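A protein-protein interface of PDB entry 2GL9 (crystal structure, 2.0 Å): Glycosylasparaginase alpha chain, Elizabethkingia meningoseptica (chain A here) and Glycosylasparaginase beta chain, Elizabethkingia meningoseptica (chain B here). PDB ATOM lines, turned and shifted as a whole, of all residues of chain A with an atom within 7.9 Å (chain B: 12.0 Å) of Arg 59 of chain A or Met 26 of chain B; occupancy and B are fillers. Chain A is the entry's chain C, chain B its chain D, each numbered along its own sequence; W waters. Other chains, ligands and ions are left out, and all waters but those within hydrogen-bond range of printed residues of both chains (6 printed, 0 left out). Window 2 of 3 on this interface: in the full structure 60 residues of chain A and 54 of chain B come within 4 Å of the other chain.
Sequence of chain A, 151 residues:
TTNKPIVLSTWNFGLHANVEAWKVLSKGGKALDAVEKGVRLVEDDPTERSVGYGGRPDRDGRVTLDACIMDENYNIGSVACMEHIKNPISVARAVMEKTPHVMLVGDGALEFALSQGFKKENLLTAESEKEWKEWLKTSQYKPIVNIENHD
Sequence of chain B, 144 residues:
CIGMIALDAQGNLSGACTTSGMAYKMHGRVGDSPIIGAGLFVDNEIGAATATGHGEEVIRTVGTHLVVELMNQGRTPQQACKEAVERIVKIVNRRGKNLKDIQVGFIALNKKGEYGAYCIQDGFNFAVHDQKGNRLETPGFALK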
ATOM      1  N   ARG A  56     -12.448  -1.158 -30.676  1.00  0.00           N
ATOM      2  CA  ARG A  56     -11.362  -1.460 -29.742  1.00  0.00           C
ATOM      3  C   ARG A  56     -11.480  -0.471 -28.574  1.00  0.00           C
ATOM      4  O   ARG A  56     -11.610   0.745 -28.771  1.00  0.00           O
ATOM      5  CB  ARG A  56     -10.008  -1.346 -30.451  1.00  0.00           C
ATOM      6  CG  ARG A  56      -9.878  -2.313 -31.649  1.00  0.00           C
ATOM      7  CD  ARG A  56      -8.429  -2.395 -32.176  1.00  0.00           C
ATOM      8  NE  ARG A  56      -8.306  -3.280 -33.334  1.00  0.00           N
ATOM      9  CZ  ARG A  56      -8.705  -2.959 -34.557  1.00  0.00           C
ATOM     10  NH1 ARG A  56      -9.249  -1.762 -34.789  1.00  0.00           N
ATOM     11  NH2 ARG A  56      -8.591  -3.840 -35.544  1.00  0.00           N
ATOM     12  N   PRO A  57     -11.447  -0.988 -27.332  1.00  0.00           N
ATOM     13  CA  PRO A  57     -11.570  -0.170 -26.121  1.00  0.00           C
ATOM     14  C   PRO A  57     -10.384   0.704 -25.815  1.00  0.00           C
ATOM     15  O   PRO A  57      -9.317   0.602 -26.455  1.00  0.00           O
ATOM     16  CB  PRO A  57     -11.787  -1.222 -25.013  1.00  0.00           C
ATOM     17  CG  PRO A  57     -10.854  -2.357 -25.484  1.00  0.00           C
ATOM     18  CD  PRO A  57     -11.159  -2.404 -26.999  1.00  0.00           C
ATOM     19  N   ASP A  58     -10.584   1.580 -24.833  1.00  0.00           N
ATOM     20  CA  ASP A  58      -9.507   2.417 -24.355  1.00  0.00           C
ATOM     21  C   ASP A  58      -8.575   1.462 -23.552  1.00  0.00           C
ATOM     22  O   ASP A  58      -8.891   0.266 -23.369  1.00  0.00           O
ATOM     23  CB  ASP A  58     -10.042   3.588 -23.497  1.00  0.00           C
ATOM     24  CG  ASP A  58     -10.744   3.148 -22.202  1.00  0.00           C
ATOM     25  OD1 ASP A  58     -11.531   3.977 -21.696  1.00  0.00           O
ATOM     26  OD2 ASP A  58     -10.511   2.023 -21.684  1.00  0.00           O
ATOM     27  N   ARG A  59      -7.439   1.973 -23.081  1.00  0.00           N
ATOM     28  CA  ARG A  59      -6.469   1.121 -22.393  1.00  0.00           C
ATOM     29  C   ARG A  59      -6.984   0.439 -21.135  1.00  0.00           C
ATOM     30  O   ARG A  59      -6.328  -0.449 -20.618  1.00  0.00           O
ATOM     31  CB  ARG A  59      -5.193   1.903 -22.073  1.00  0.00           C
ATOM     32  CG  ARG A  59      -5.369   2.965 -21.012  1.00  0.00           C
ATOM     33  CD  ARG A  59      -4.088   3.761 -20.873  1.00  0.00           C
ATOM     34  NE  ARG A  59      -4.164   4.751 -19.798  1.00  0.00           N
ATOM     35  CZ  ARG A  59      -3.129   5.482 -19.378  1.00  0.00           C
ATOM     36  NH1 ARG A  59      -1.936   5.331 -19.948  1.00  0.00           N
ATOM     37  NH2 ARG A  59      -3.283   6.347 -18.377  1.00  0.00           N
ATOM     38  N   ASP A  60      -8.147   0.850 -20.649  1.00  0.00           N
ATOM     39  CA  ASP A  60      -8.724   0.212 -19.475  1.00  0.00           C
ATOM     40  C   ASP A  60      -9.813  -0.798 -19.829  1.00  0.00           C
ATOM     41  O   ASP A  60     -10.474  -1.336 -18.936  1.00  0.00           O
ATOM     42  CB  ASP A  60      -9.269   1.265 -18.514  1.00  0.00           C
ATOM     43  CG  ASP A  60      -8.185   2.175 -18.005  1.00  0.00           C
ATOM     44  OD1 ASP A  60      -7.114   1.659 -17.571  1.00  0.00           O
ATOM     45  OD2 ASP A  60      -8.385   3.401 -18.051  1.00  0.00           O
ATOM     46  N   GLY A  61      -9.976  -1.069 -21.128  1.00  0.00           N
ATOM     47  CA  GLY A  61     -10.982  -2.015 -21.603  1.00  0.00           C
ATOM     48  C   GLY A  61     -12.397  -1.475 -21.786  1.00  0.00           C
ATOM     49  O   GLY A  61     -13.363  -2.252 -21.961  1.00  0.00           O
ATOM     50  N   ARG A  62     -12.550  -0.148 -21.755  1.00  0.00           N
ATOM     51  CA  ARG A  62     -13.870   0.430 -21.907  1.00  0.00           C
ATOM     52  C   ARG A  62     -14.089   0.891 -23.326  1.00  0.00           C
ATOM     53  O   ARG A  62     -13.262   1.608 -23.887  1.00  0.00           O
ATOM     54  CB  ARG A  62     -14.037   1.596 -20.928  1.00  0.00           C
ATOM     55  CG  ARG A  62     -14.032   1.095 -19.498  1.00  0.00           C
ATOM     56  CD  ARG A  62     -13.878   2.184 -18.471  1.00  0.00           C
ATOM     57  NE  ARG A  62     -14.951   3.172 -18.527  1.00  0.00           N
ATOM     58  CZ  ARG A  62     -15.224   4.018 -17.540  1.00  0.00           C
ATOM     59  NH1 ARG A  62     -14.498   3.968 -16.428  1.00  0.00           N
ATOM     60  NH2 ARG A  62     -16.188   4.933 -17.677  1.00  0.00           N
ATOM     61  N   THR A  64     -15.484   3.409 -25.574  1.00  0.00           N
ATOM     62  CA  THR A  64     -16.153   4.712 -25.513  1.00  0.00           C
ATOM     63  C   THR A  64     -16.202   5.320 -26.931  1.00  0.00           C
ATOM     64  O   THR A  64     -15.202   5.371 -27.623  1.00  0.00           O
ATOM     65  CB  THR A  64     -15.463   5.668 -24.504  1.00  0.00           C
ATOM     66  OG1 THR A  64     -14.237   6.168 -25.051  1.00  0.00           O
ATOM     67  CG2 THR A  64     -15.181   4.912 -23.165  1.00  0.00           C
ATOM     68  N   CYS A  81     -17.103  10.220 -25.860  1.00  0.00           N
ATOM     69  CA  CYS A  81     -16.770   9.318 -24.765  1.00  0.00           C
ATOM     70  C   CYS A  81     -18.051   8.758 -24.118  1.00  0.00           C
ATOM     71  O   CYS A  81     -18.265   8.850 -22.897  1.00  0.00           O
ATOM     72  CB  CYS A  81     -15.907  10.047 -23.731  1.00  0.00           C
ATOM     73  SG  CYS A  81     -15.075   8.882 -22.599  1.00  0.00           S
ATOM     74  N   TRP A 132      -7.352  -6.670 -26.770  1.00  0.00           N
ATOM     75  CA  TRP A 132      -7.028  -5.700 -25.732  1.00  0.00           C
ATOM     76  C   TRP A 132      -6.067  -6.349 -24.750  1.00  0.00           C
ATOM     77  O   TRP A 132      -5.007  -5.797 -24.436  1.00  0.00           O
ATOM     78  CB  TRP A 132      -8.309  -5.253 -25.004  1.00  0.00           C
ATOM     79  CG  TRP A 132      -8.058  -4.446 -23.773  1.00  0.00           C
ATOM     80  CD1 TRP A 132      -7.273  -3.335 -23.670  1.00  0.00           C
ATOM     81  CD2 TRP A 132      -8.558  -4.709 -22.456  1.00  0.00           C
ATOM     82  NE1 TRP A 132      -7.244  -2.890 -22.366  1.00  0.00           N
ATOM     83  CE2 TRP A 132      -8.025  -3.714 -21.601  1.00  0.00           C
ATOM     84  CE3 TRP A 132      -9.398  -5.688 -21.914  1.00  0.00           C
ATOM     85  CZ2 TRP A 132      -8.309  -3.673 -20.236  1.00  0.00           C
ATOM     86  CZ3 TRP A 132      -9.683  -5.648 -20.548  1.00  0.00           C
ATOM     87  CH2 TRP A 132      -9.140  -4.647 -19.723  1.00  0.00           C
ATOM     88  N   TRP A 135      -2.645  -6.692 -25.961  1.00  0.00           N
ATOM     89  CA  TRP A 135      -1.961  -5.403 -25.973  1.00  0.00           C
ATOM     90  C   TRP A 135      -1.426  -5.104 -24.575  1.00  0.00           C
ATOM     91  O   TRP A 135      -0.338  -4.530 -24.404  1.00  0.00           O
ATOM     92  CB  TRP A 135      -2.923  -4.277 -26.386  1.00  0.00           C
ATOM     93  CG  TRP A 135      -2.303  -2.889 -26.283  1.00  0.00           C
ATOM     94  CD1 TRP A 135      -1.421  -2.320 -27.160  1.00  0.00           C
ATOM     95  CD2 TRP A 135      -2.467  -1.943 -25.210  1.00  0.00           C
ATOM     96  NE1 TRP A 135      -1.024  -1.079 -26.700  1.00  0.00           N
ATOM     97  CE2 TRP A 135      -1.658  -0.823 -25.508  1.00  0.00           C
ATOM     98  CE3 TRP A 135      -3.223  -1.935 -24.028  1.00  0.00           C
ATOM     99  CZ2 TRP A 135      -1.582   0.298 -24.665  1.00  0.00           C
ATOM    100  CZ3 TRP A 135      -3.151  -0.832 -23.192  1.00  0.00           C
ATOM    101  CH2 TRP A 135      -2.334   0.277 -23.515  1.00  0.00           C
ATOM    102  N   LEU A 136      -2.213  -5.468 -23.576  1.00  0.00           N
ATOM    103  CA  LEU A 136      -1.803  -5.236 -22.200  1.00  0.00           C
ATOM    104  C   LEU A 136      -0.486  -5.969 -21.956  1.00  0.00           C
ATOM    105  O   LEU A 136       0.400  -5.466 -21.265  1.00  0.00           O
ATOM    106  CB  LEU A 136      -2.873  -5.742 -21.234  1.00  0.00           C
ATOM    107  CG  LEU A 136      -4.156  -4.918 -21.086  1.00  0.00           C
ATOM    108  CD1 LEU A 136      -5.141  -5.689 -20.218  1.00  0.00           C
ATOM    109  CD2 LEU A 136      -3.850  -3.549 -20.466  1.00  0.00           C
ATOM    110  N   SER A 139       2.368  -4.031 -24.081  1.00  0.00           N
ATOM    111  CA  SER A 139       2.570  -2.677 -23.596  1.00  0.00           C
ATOM    112  C   SER A 139       2.936  -2.674 -22.130  1.00  0.00           C
ATOM    113  O   SER A 139       3.572  -1.735 -21.642  1.00  0.00           O
ATOM    114  CB  SER A 139       1.294  -1.849 -23.761  1.00  0.00           C
ATOM    115  OG  SER A 139       0.417  -2.045 -22.661  1.00  0.00           O
ATOM    116  N   TYR A 141       0.925  -2.165 -19.689  1.00  0.00           N
ATOM    117  CA  TYR A 141       0.166  -1.127 -18.964  1.00  0.00           C
ATOM    118  C   TYR A 141      -0.704  -1.792 -17.895  1.00  0.00           C
ATOM    119  O   TYR A 141      -1.278  -2.861 -18.129  1.00  0.00           O
ATOM    120  CB  TYR A 141      -0.735  -0.334 -19.935  1.00  0.00           C
ATOM    121  CG  TYR A 141      -1.798   0.523 -19.253  1.00  0.00           C
ATOM    122  CD1 TYR A 141      -1.470   1.725 -18.632  1.00  0.00           C
ATOM    123  CD2 TYR A 141      -3.133   0.089 -19.187  1.00  0.00           C
ATOM    124  CE1 TYR A 141      -2.444   2.479 -17.951  1.00  0.00           C
ATOM    125  CE2 TYR A 141      -4.117   0.830 -18.515  1.00  0.00           C
ATOM    126  CZ  TYR A 141      -3.766   2.014 -17.901  1.00  0.00           C
ATOM    127  OH  TYR A 141      -4.740   2.719 -17.222  1.00  0.00           O
ATOM    128  N   LYS A 142      -0.792  -1.164 -16.726  1.00  0.00           N
ATOM    129  CA  LYS A 142      -1.612  -1.685 -15.625  1.00  0.00           C
ATOM    130  C   LYS A 142      -2.943  -0.936 -15.514  1.00  0.00           C
ATOM    131  O   LYS A 142      -2.975   0.192 -15.023  1.00  0.00           O
ATOM    132  CB  LYS A 142      -0.885  -1.526 -14.283  1.00  0.00           C
ATOM    133  CG  LYS A 142       0.408  -2.313 -14.117  1.00  0.00           C
ATOM    134  CD  LYS A 142       1.563  -1.749 -14.946  1.00  0.00           C
ATOM    135  CE  LYS A 142       2.874  -2.458 -14.584  1.00  0.00           C
ATOM    136  NZ  LYS A 142       2.702  -3.950 -14.546  1.00  0.00           N
ATOM    137  N   PRO A 143      -4.064  -1.551 -15.948  1.00  0.00           N
ATOM    138  CA  PRO A 143      -5.365  -0.859 -15.858  1.00  0.00           C
ATOM    139  C   PRO A 143      -5.952  -0.676 -14.444  1.00  0.00           C
ATOM    140  O   PRO A 143      -5.438  -1.310 -13.493  1.00  0.00           O
ATOM    141  CB  PRO A 143      -6.270  -1.700 -16.770  1.00  0.00           C
ATOM    142  CG  PRO A 143      -5.669  -3.060 -16.688  1.00  0.00           C
ATOM    143  CD  PRO A 143      -4.182  -2.791 -16.738  1.00  0.00           C
ATOM    144  N   THR B  19     -16.959   7.135 -34.449  1.00  0.00           N
ATOM    145  CA  THR B  19     -15.779   6.311 -34.211  1.00  0.00           C
ATOM    146  C   THR B  19     -15.705   5.733 -32.799  1.00  0.00           C
ATOM    147  O   THR B  19     -16.377   6.199 -31.885  1.00  0.00           O
ATOM    148  CB  THR B  19     -14.467   7.175 -34.433  1.00  0.00           C
ATOM    149  OG1 THR B  19     -13.292   6.353 -34.341  1.00  0.00           O
ATOM    150  CG2 THR B  19     -14.345   8.259 -33.353  1.00  0.00           C
ATOM    151  N   SER B  20     -14.839   4.740 -32.625  1.00  0.00           N
ATOM    152  CA  SER B  20     -14.600   4.185 -31.313  1.00  0.00           C
ATOM    153  C   SER B  20     -13.279   4.789 -30.861  1.00  0.00           C
ATOM    154  O   SER B  20     -12.781   4.519 -29.761  1.00  0.00           O
ATOM    155  CB  SER B  20     -14.509   2.672 -31.369  1.00  0.00           C
ATOM    156  OG  SER B  20     -13.451   2.280 -32.195  1.00  0.00           O
ATOM    157  N   GLY B  21     -12.705   5.620 -31.729  1.00  0.00           N
ATOM    158  CA  GLY B  21     -11.469   6.306 -31.389  1.00  0.00           C
ATOM    159  C   GLY B  21     -10.187   5.494 -31.489  1.00  0.00           C
ATOM    160  O   GLY B  21     -10.205   4.354 -31.907  1.00  0.00           O
ATOM    161  N   MET B  22      -9.076   6.123 -31.125  1.00  0.00           N
ATOM    162  CA  MET B  22      -7.755   5.498 -31.153  1.00  0.00           C
ATOM    163  C   MET B  22      -7.719   4.326 -30.166  1.00  0.00           C
ATOM    164  O   MET B  22      -7.970   4.492 -28.976  1.00  0.00           O
ATOM    165  CB  MET B  22      -6.673   6.514 -30.748  1.00  0.00           C
ATOM    166  CG  MET B  22      -5.266   5.931 -30.689  1.00  0.00           C
ATOM    167  SD  MET B  22      -4.090   6.869 -29.609  1.00  0.00           S
ATOM    168  CE  MET B  22      -4.340   8.529 -30.319  1.00  0.00           C
ATOM    169  N   ALA B  23      -7.413   3.146 -30.680  1.00  0.00           N
ATOM    170  CA  ALA B  23      -7.337   1.944 -29.851  1.00  0.00           C
ATOM    171  C   ALA B  23      -6.386   2.125 -28.643  1.00  0.00           C
ATOM    172  O   ALA B  23      -5.291   2.658 -28.769  1.00  0.00           O
ATOM    173  CB  ALA B  23      -6.889   0.769 -30.716  1.00  0.00           C
ATOM    174  N   TYR B  24      -6.858   1.733 -27.464  1.00  0.00           N
ATOM    175  CA  TYR B  24      -6.072   1.794 -26.234  1.00  0.00           C
ATOM    176  C   TYR B  24      -5.700   3.201 -25.755  1.00  0.00           C
ATOM    177  O   TYR B  24      -4.732   3.382 -25.014  1.00  0.00           O
ATOM    178  CB  TYR B  24      -4.844   0.900 -26.413  1.00  0.00           C
ATOM    179  CG  TYR B  24      -5.238  -0.430 -27.053  1.00  0.00           C
ATOM    180  CD1 TYR B  24      -4.493  -0.983 -28.091  1.00  0.00           C
ATOM    181  CD2 TYR B  24      -6.399  -1.094 -26.647  1.00  0.00           C
ATOM    182  CE1 TYR B  24      -4.902  -2.182 -28.725  1.00  0.00           C
ATOM    183  CE2 TYR B  24      -6.820  -2.270 -27.269  1.00  0.00           C
ATOM    184  CZ  TYR B  24      -6.071  -2.811 -28.308  1.00  0.00           C
ATOM    185  OH  TYR B  24      -6.525  -3.963 -28.940  1.00  0.00           O
ATOM    186  N   LYS B  25      -6.510   4.183 -26.176  1.00  0.00           N
ATOM    187  CA  LYS B  25      -6.370   5.591 -25.805  1.00  0.00           C
ATOM    188  C   LYS B  25      -6.498   5.708 -24.294  1.00  0.00           C
ATOM    189  O   LYS B  25      -7.007   4.792 -23.619  1.00  0.00           O
ATOM    190  CB  LYS B  25      -7.517   6.421 -26.429  1.00  0.00           C
ATOM    191  CG  LYS B  25      -8.901   5.926 -25.973  1.00  0.00           C
ATOM    192  CD  LYS B  25     -10.061   6.457 -26.820  1.00  0.00           C
ATOM    193  CE  LYS B  25     -11.382   5.751 -26.461  1.00  0.00           C
ATOM    194  NZ  LYS B  25     -12.530   6.050 -27.444  1.00  0.00           N
ATOM    195  N   MET B  26      -6.063   6.844 -23.757  1.00  0.00           N
ATOM    196  CA  MET B  26      -6.245   7.080 -22.326  1.00  0.00           C
ATOM    197  C   MET B  26      -7.751   7.137 -22.058  1.00  0.00           C
ATOM    198  O   MET B  26      -8.515   7.580 -22.928  1.00  0.00           O
ATOM    199  CB  MET B  26      -5.633   8.411 -21.937  1.00  0.00           C
ATOM    200  CG  MET B  26      -4.167   8.268 -21.633  1.00  0.00           C
ATOM    201  SD  MET B  26      -3.396   9.799 -21.252  1.00  0.00           S
ATOM    202  CE  MET B  26      -4.036  10.133 -19.607  1.00  0.00           C
ATOM    203  N   HIS B  27      -8.189   6.709 -20.871  1.00  0.00           N
ATOM    204  CA  HIS B  27      -9.612   6.778 -20.573  1.00  0.00           C
ATOM    205  C   HIS B  27     -10.065   8.253 -20.677  1.00  0.00           C
ATOM    206  O   HIS B  27      -9.411   9.155 -20.141  1.00  0.00           O
ATOM    207  CB  HIS B  27      -9.893   6.215 -19.172  1.00  0.00           C
ATOM    208  CG  HIS B  27     -11.344   6.212 -18.808  1.00  0.00           C
ATOM    209  ND1 HIS B  27     -12.313   5.685 -19.636  1.00  0.00           N
ATOM    210  CD2 HIS B  27     -12.003   6.749 -17.755  1.00  0.00           C
ATOM    211  CE1 HIS B  27     -13.505   5.916 -19.120  1.00  0.00           C
ATOM    212  NE2 HIS B  27     -13.346   6.561 -17.981  1.00  0.00           N
ATOM    213  N   GLY B  28     -11.173   8.501 -21.372  1.00  0.00           N
ATOM    214  CA  GLY B  28     -11.662   9.871 -21.510  1.00  0.00           C
ATOM    215  C   GLY B  28     -11.071  10.628 -22.708  1.00  0.00           C
ATOM    216  O   GLY B  28     -11.408  11.797 -22.966  1.00  0.00           O
ATOM    217  N   ARG B  29     -10.209   9.972 -23.472  1.00  0.00           N
ATOM    218  CA  ARG B  29      -9.607  10.660 -24.619  1.00  0.00           C
ATOM    219  C   ARG B  29     -10.623  10.891 -25.712  1.00  0.00           C
ATOM    220  O   ARG B  29     -11.424  10.002 -26.043  1.00  0.00           O
ATOM    221  CB  ARG B  29      -8.415   9.883 -25.175  1.00  0.00           C
ATOM    222  CG  ARG B  29      -7.781  10.478 -26.463  1.00  0.00           C
ATOM    223  CD  ARG B  29      -8.538  10.004 -27.702  1.00  0.00           C
ATOM    224  NE  ARG B  29      -7.847  10.357 -28.945  1.00  0.00           N
ATOM    225  CZ  ARG B  29      -8.321  10.066 -30.158  1.00  0.00           C
ATOM    226  NH1 ARG B  29      -9.491   9.425 -30.292  1.00  0.00           N
ATOM    227  NH2 ARG B  29      -7.621  10.397 -31.237  1.00  0.00           N
ATOM    228  N   VAL B  30     -10.611  12.105 -26.255  1.00  0.00           N
ATOM    229  CA  VAL B  30     -11.535  12.432 -27.329  1.00  0.00           C
ATOM    230  C   VAL B  30     -10.747  12.927 -28.551  1.00  0.00           C
ATOM    231  O   VAL B  30      -9.841  13.774 -28.424  1.00  0.00           O
ATOM    232  CB  VAL B  30     -12.552  13.547 -26.903  1.00  0.00           C
ATOM    233  CG1 VAL B  30     -13.348  13.996 -28.114  1.00  0.00           C
ATOM    234  CG2 VAL B  30     -13.515  13.025 -25.831  1.00  0.00           C
ATOM    235  N   GLY B  31     -11.063  12.374 -29.718  1.00  0.00           N
ATOM    236  CA  GLY B  31     -10.401  12.803 -30.940  1.00  0.00           C
ATOM    237  C   GLY B  31     -11.210  13.872 -31.694  1.00  0.00           C
ATOM    238  O   GLY B  31     -12.026  14.575 -31.106  1.00  0.00           O
ATOM    239  N   GLU B  56      -5.872  14.008 -33.041  1.00  0.00           N
ATOM    240  CA  GLU B  56      -5.167  15.076 -32.353  1.00  0.00           C
ATOM    241  C   GLU B  56      -4.708  16.158 -33.334  1.00  0.00           C
ATOM    242  O   GLU B  56      -4.821  17.356 -33.046  1.00  0.00           O
ATOM    243  CB  GLU B  56      -3.956  14.498 -31.576  1.00  0.00           C
ATOM    244  CG  GLU B  56      -4.283  13.883 -30.208  1.00  0.00           C
ATOM    245  CD  GLU B  56      -4.991  12.516 -30.267  1.00  0.00           C
ATOM    246  OE1 GLU B  56      -5.059  11.881 -31.355  1.00  0.00           O
ATOM    247  OE2 GLU B  56      -5.482  12.090 -29.198  1.00  0.00           O
HETATM  248  O   HOH W   1      -6.810   5.323 -18.677  1.00  0.00           O
HETATM  249  O   HOH W   2     -13.384   2.823 -27.441  1.00  0.00           O
HETATM  250  O   HOH W   3     -12.213   6.353 -22.913  1.00  0.00           O
HETATM  251  O   HOH W   4     -13.963   9.531 -19.033  1.00  0.00           O
HETATM  252  O   HOH W   5     -13.873   8.490 -26.235  1.00  0.00           O
HETATM  253  O   HOH W   6     -11.274   1.799 -31.080  1.00  0.00           O
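The backbone NH (N) of Tyr 24 of chain B lies within hydrogen-bond range of the backbone carbonyl oxygen (O) of Pro 57 of chain A.
ND1 of His 27 of chain B lies within hydrogen-bond range of OD1 of Asp 58 of chain A (2.8 Å).
N of Arg 59 of chain A lies within hydrogen-bond range of O of Lys 25 of chain B (2.9 Å).
The guanidinium group (NH1) of Arg 62 of chain A lies close to a ring nitrogen (NE2) of His 27 of chain B (3.2 Å).
O of Thr 64 of chain A lies within hydrogen-bond range of NZ of Lys 25 of chain B.
O of Thr 64 of chain A lies close to O of Ser 20 of chain B (3.3 Å).
The backbone carbonyl oxygen (O) of Arg 59 of chain A sits at hydrogen-bond distance from the indole nitrogen (NE1) of Trp 132 of chain A, at 3.1 Å.
The guanidinium group of Arg 59 of chain A sits at hydrogen-bond distance from the side-chain hydroxyl of Tyr 141 of chain A (3.3 Å).
The side-chain carboxylate (OD1) of Asp 60 of chain A sits at hydrogen-bond distance from the side-chain hydroxyl (OH) of Tyr 141 of chain A, at 2.6 Å.
The side-chain sulfur (SG) of Cys 81 of chain A lies within hydrogen-bond range of the side-chain hydroxyl (OG1) of Thr 64 of chain A.
The backbone carbonyl oxygen (O) of Trp 135 of chain A sits at hydrogen-bond distance from the side-chain hydroxyl (OG) of Ser 139 of chain A (3.1 Å).
The backbone carbonyl oxygen (O) of Ser 20 of chain B sits at hydrogen-bond distance from the side-chain amino group (NZ) of Lys 25 of chain B (2.8 Å).
Among the printed residues, merely in contact across the chains: Asp 58 of chain A with Lys 25 of chain B, Arg 59 of chain A with Tyr 24 of chain B, Asp 60 of chain A with His 27 of chain B, Trp 135 of chain A with Tyr 24 of chain B, Trp 132 of chain A with Tyr 24 of chain B, Asp 58 of chain A with Tyr 24 of chain B, Cys 81 of chain A with Gly 28 of chain B, Arg 59 of chain A with Met 26 of chain B, Arg 56 of chain A with Ala 23 of chain B, Arg 56 of chain A with Ser 20 of chain B and Pro 57 of chain A with Ala 23 of chain B.
Of the printed residues of chain A, Met 26 of chain B touches Arg 59.
Of chain B, only Ala 23 and Tyr 24 come within 4 Å of Pro 57 of chain A.
Asp 58 of chain A touches just these residues of chain B: Tyr 24 (3.7 Å), Lys 25 (3.3 Å) and His 27 (2.8 Å).
Of chain B, only His 27 (3.4 Å) comes within 4 Å of Asp 60 of chain A.
No residue of chain B comes within 4 Å of Gly 61 of chain A.
No residue of chain B comes within 4 Å of Tyr 141 of chain A.
No residue of chain B comes within 4 Å of Pro 143 of chain A.
Of the printed residues of chain A, Ala 23 of chain B touches Arg 56 and Pro 57.
Of the printed residues of chain A, His 27 of chain B touches Asp 58 (2.8 Å), Asp 60 (3.4 Å) and Arg 62 (3.0 Å).
Printed residues of chain B within 4 Å of Thr 64 of chain A: Ser 20 (3.3 Å) and Lys 25 (2.8 Å).
Of the printed residues of chain A, Ser 20 of chain B touches Arg 56 and Thr 64.
Of the printed residues of chain A, Gly 28 of chain B touches Cys 81.
Thr 19 of chain B touches none of the printed residues of chain A.
Leu 136 of chain A touches none of the printed residues of chain B.
The nearest printed residue of chain B that does not touch Thr 64 of chain A is His 27 of chain B (4.5 Å).
Of the 14 printed residues of chain B, 7 touch a printed residue of chain A.
Of the 16 printed residues of chain A, 10 touch a printed residue of chain B.
Along chain A the printed residues that touch a printed residue of chain B span positions 56 to 135.
Water W6 lies within hydrogen-bond range of the side-chain hydroxyl (OG) of Ser 20 of chain B (2.5 Å), the backbone carbonyl oxygen (O) of Arg 56 of chain A (2.6 Å) and the backbone carbonyl oxygen (O) of Gly 21 of chain B (2.9 Å).
Water W1 lies within hydrogen-bond range of the side-chain carboxylate (OD2) of Asp 60 of chain A (2.6 Å), the guanidinium group (NE) of Arg 59 of chain A (2.9 Å) and the backbone NH (N) of His 27 of chain B (2.9 Å).
Water W5 lies within hydrogen-bond range of OG1 of Thr 64 of chain A, O of Arg 29 of chain B and NZ of Lys 25 of chain B.
Water W3 lies within hydrogen-bond range of the side-chain carboxylate (OD1) of Asp 58 of chain A, the backbone NH (N) of Gly 28 of chain B, the side-chain hydroxyl (OG1) of Thr 64 of chain A and a ring nitrogen (ND1) of His 27 of chain B.
Water W2 lies within hydrogen-bond range of N of Thr 64 of chain A, O of Ser 20 of chain B, O of Arg 56 of chain A and NZ of Lys 25 of chain B.
Water W4 bridges NE2 of His 27 of chain B (3.2 Å) and SG of Cys 81 of chain A (3.8 Å).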
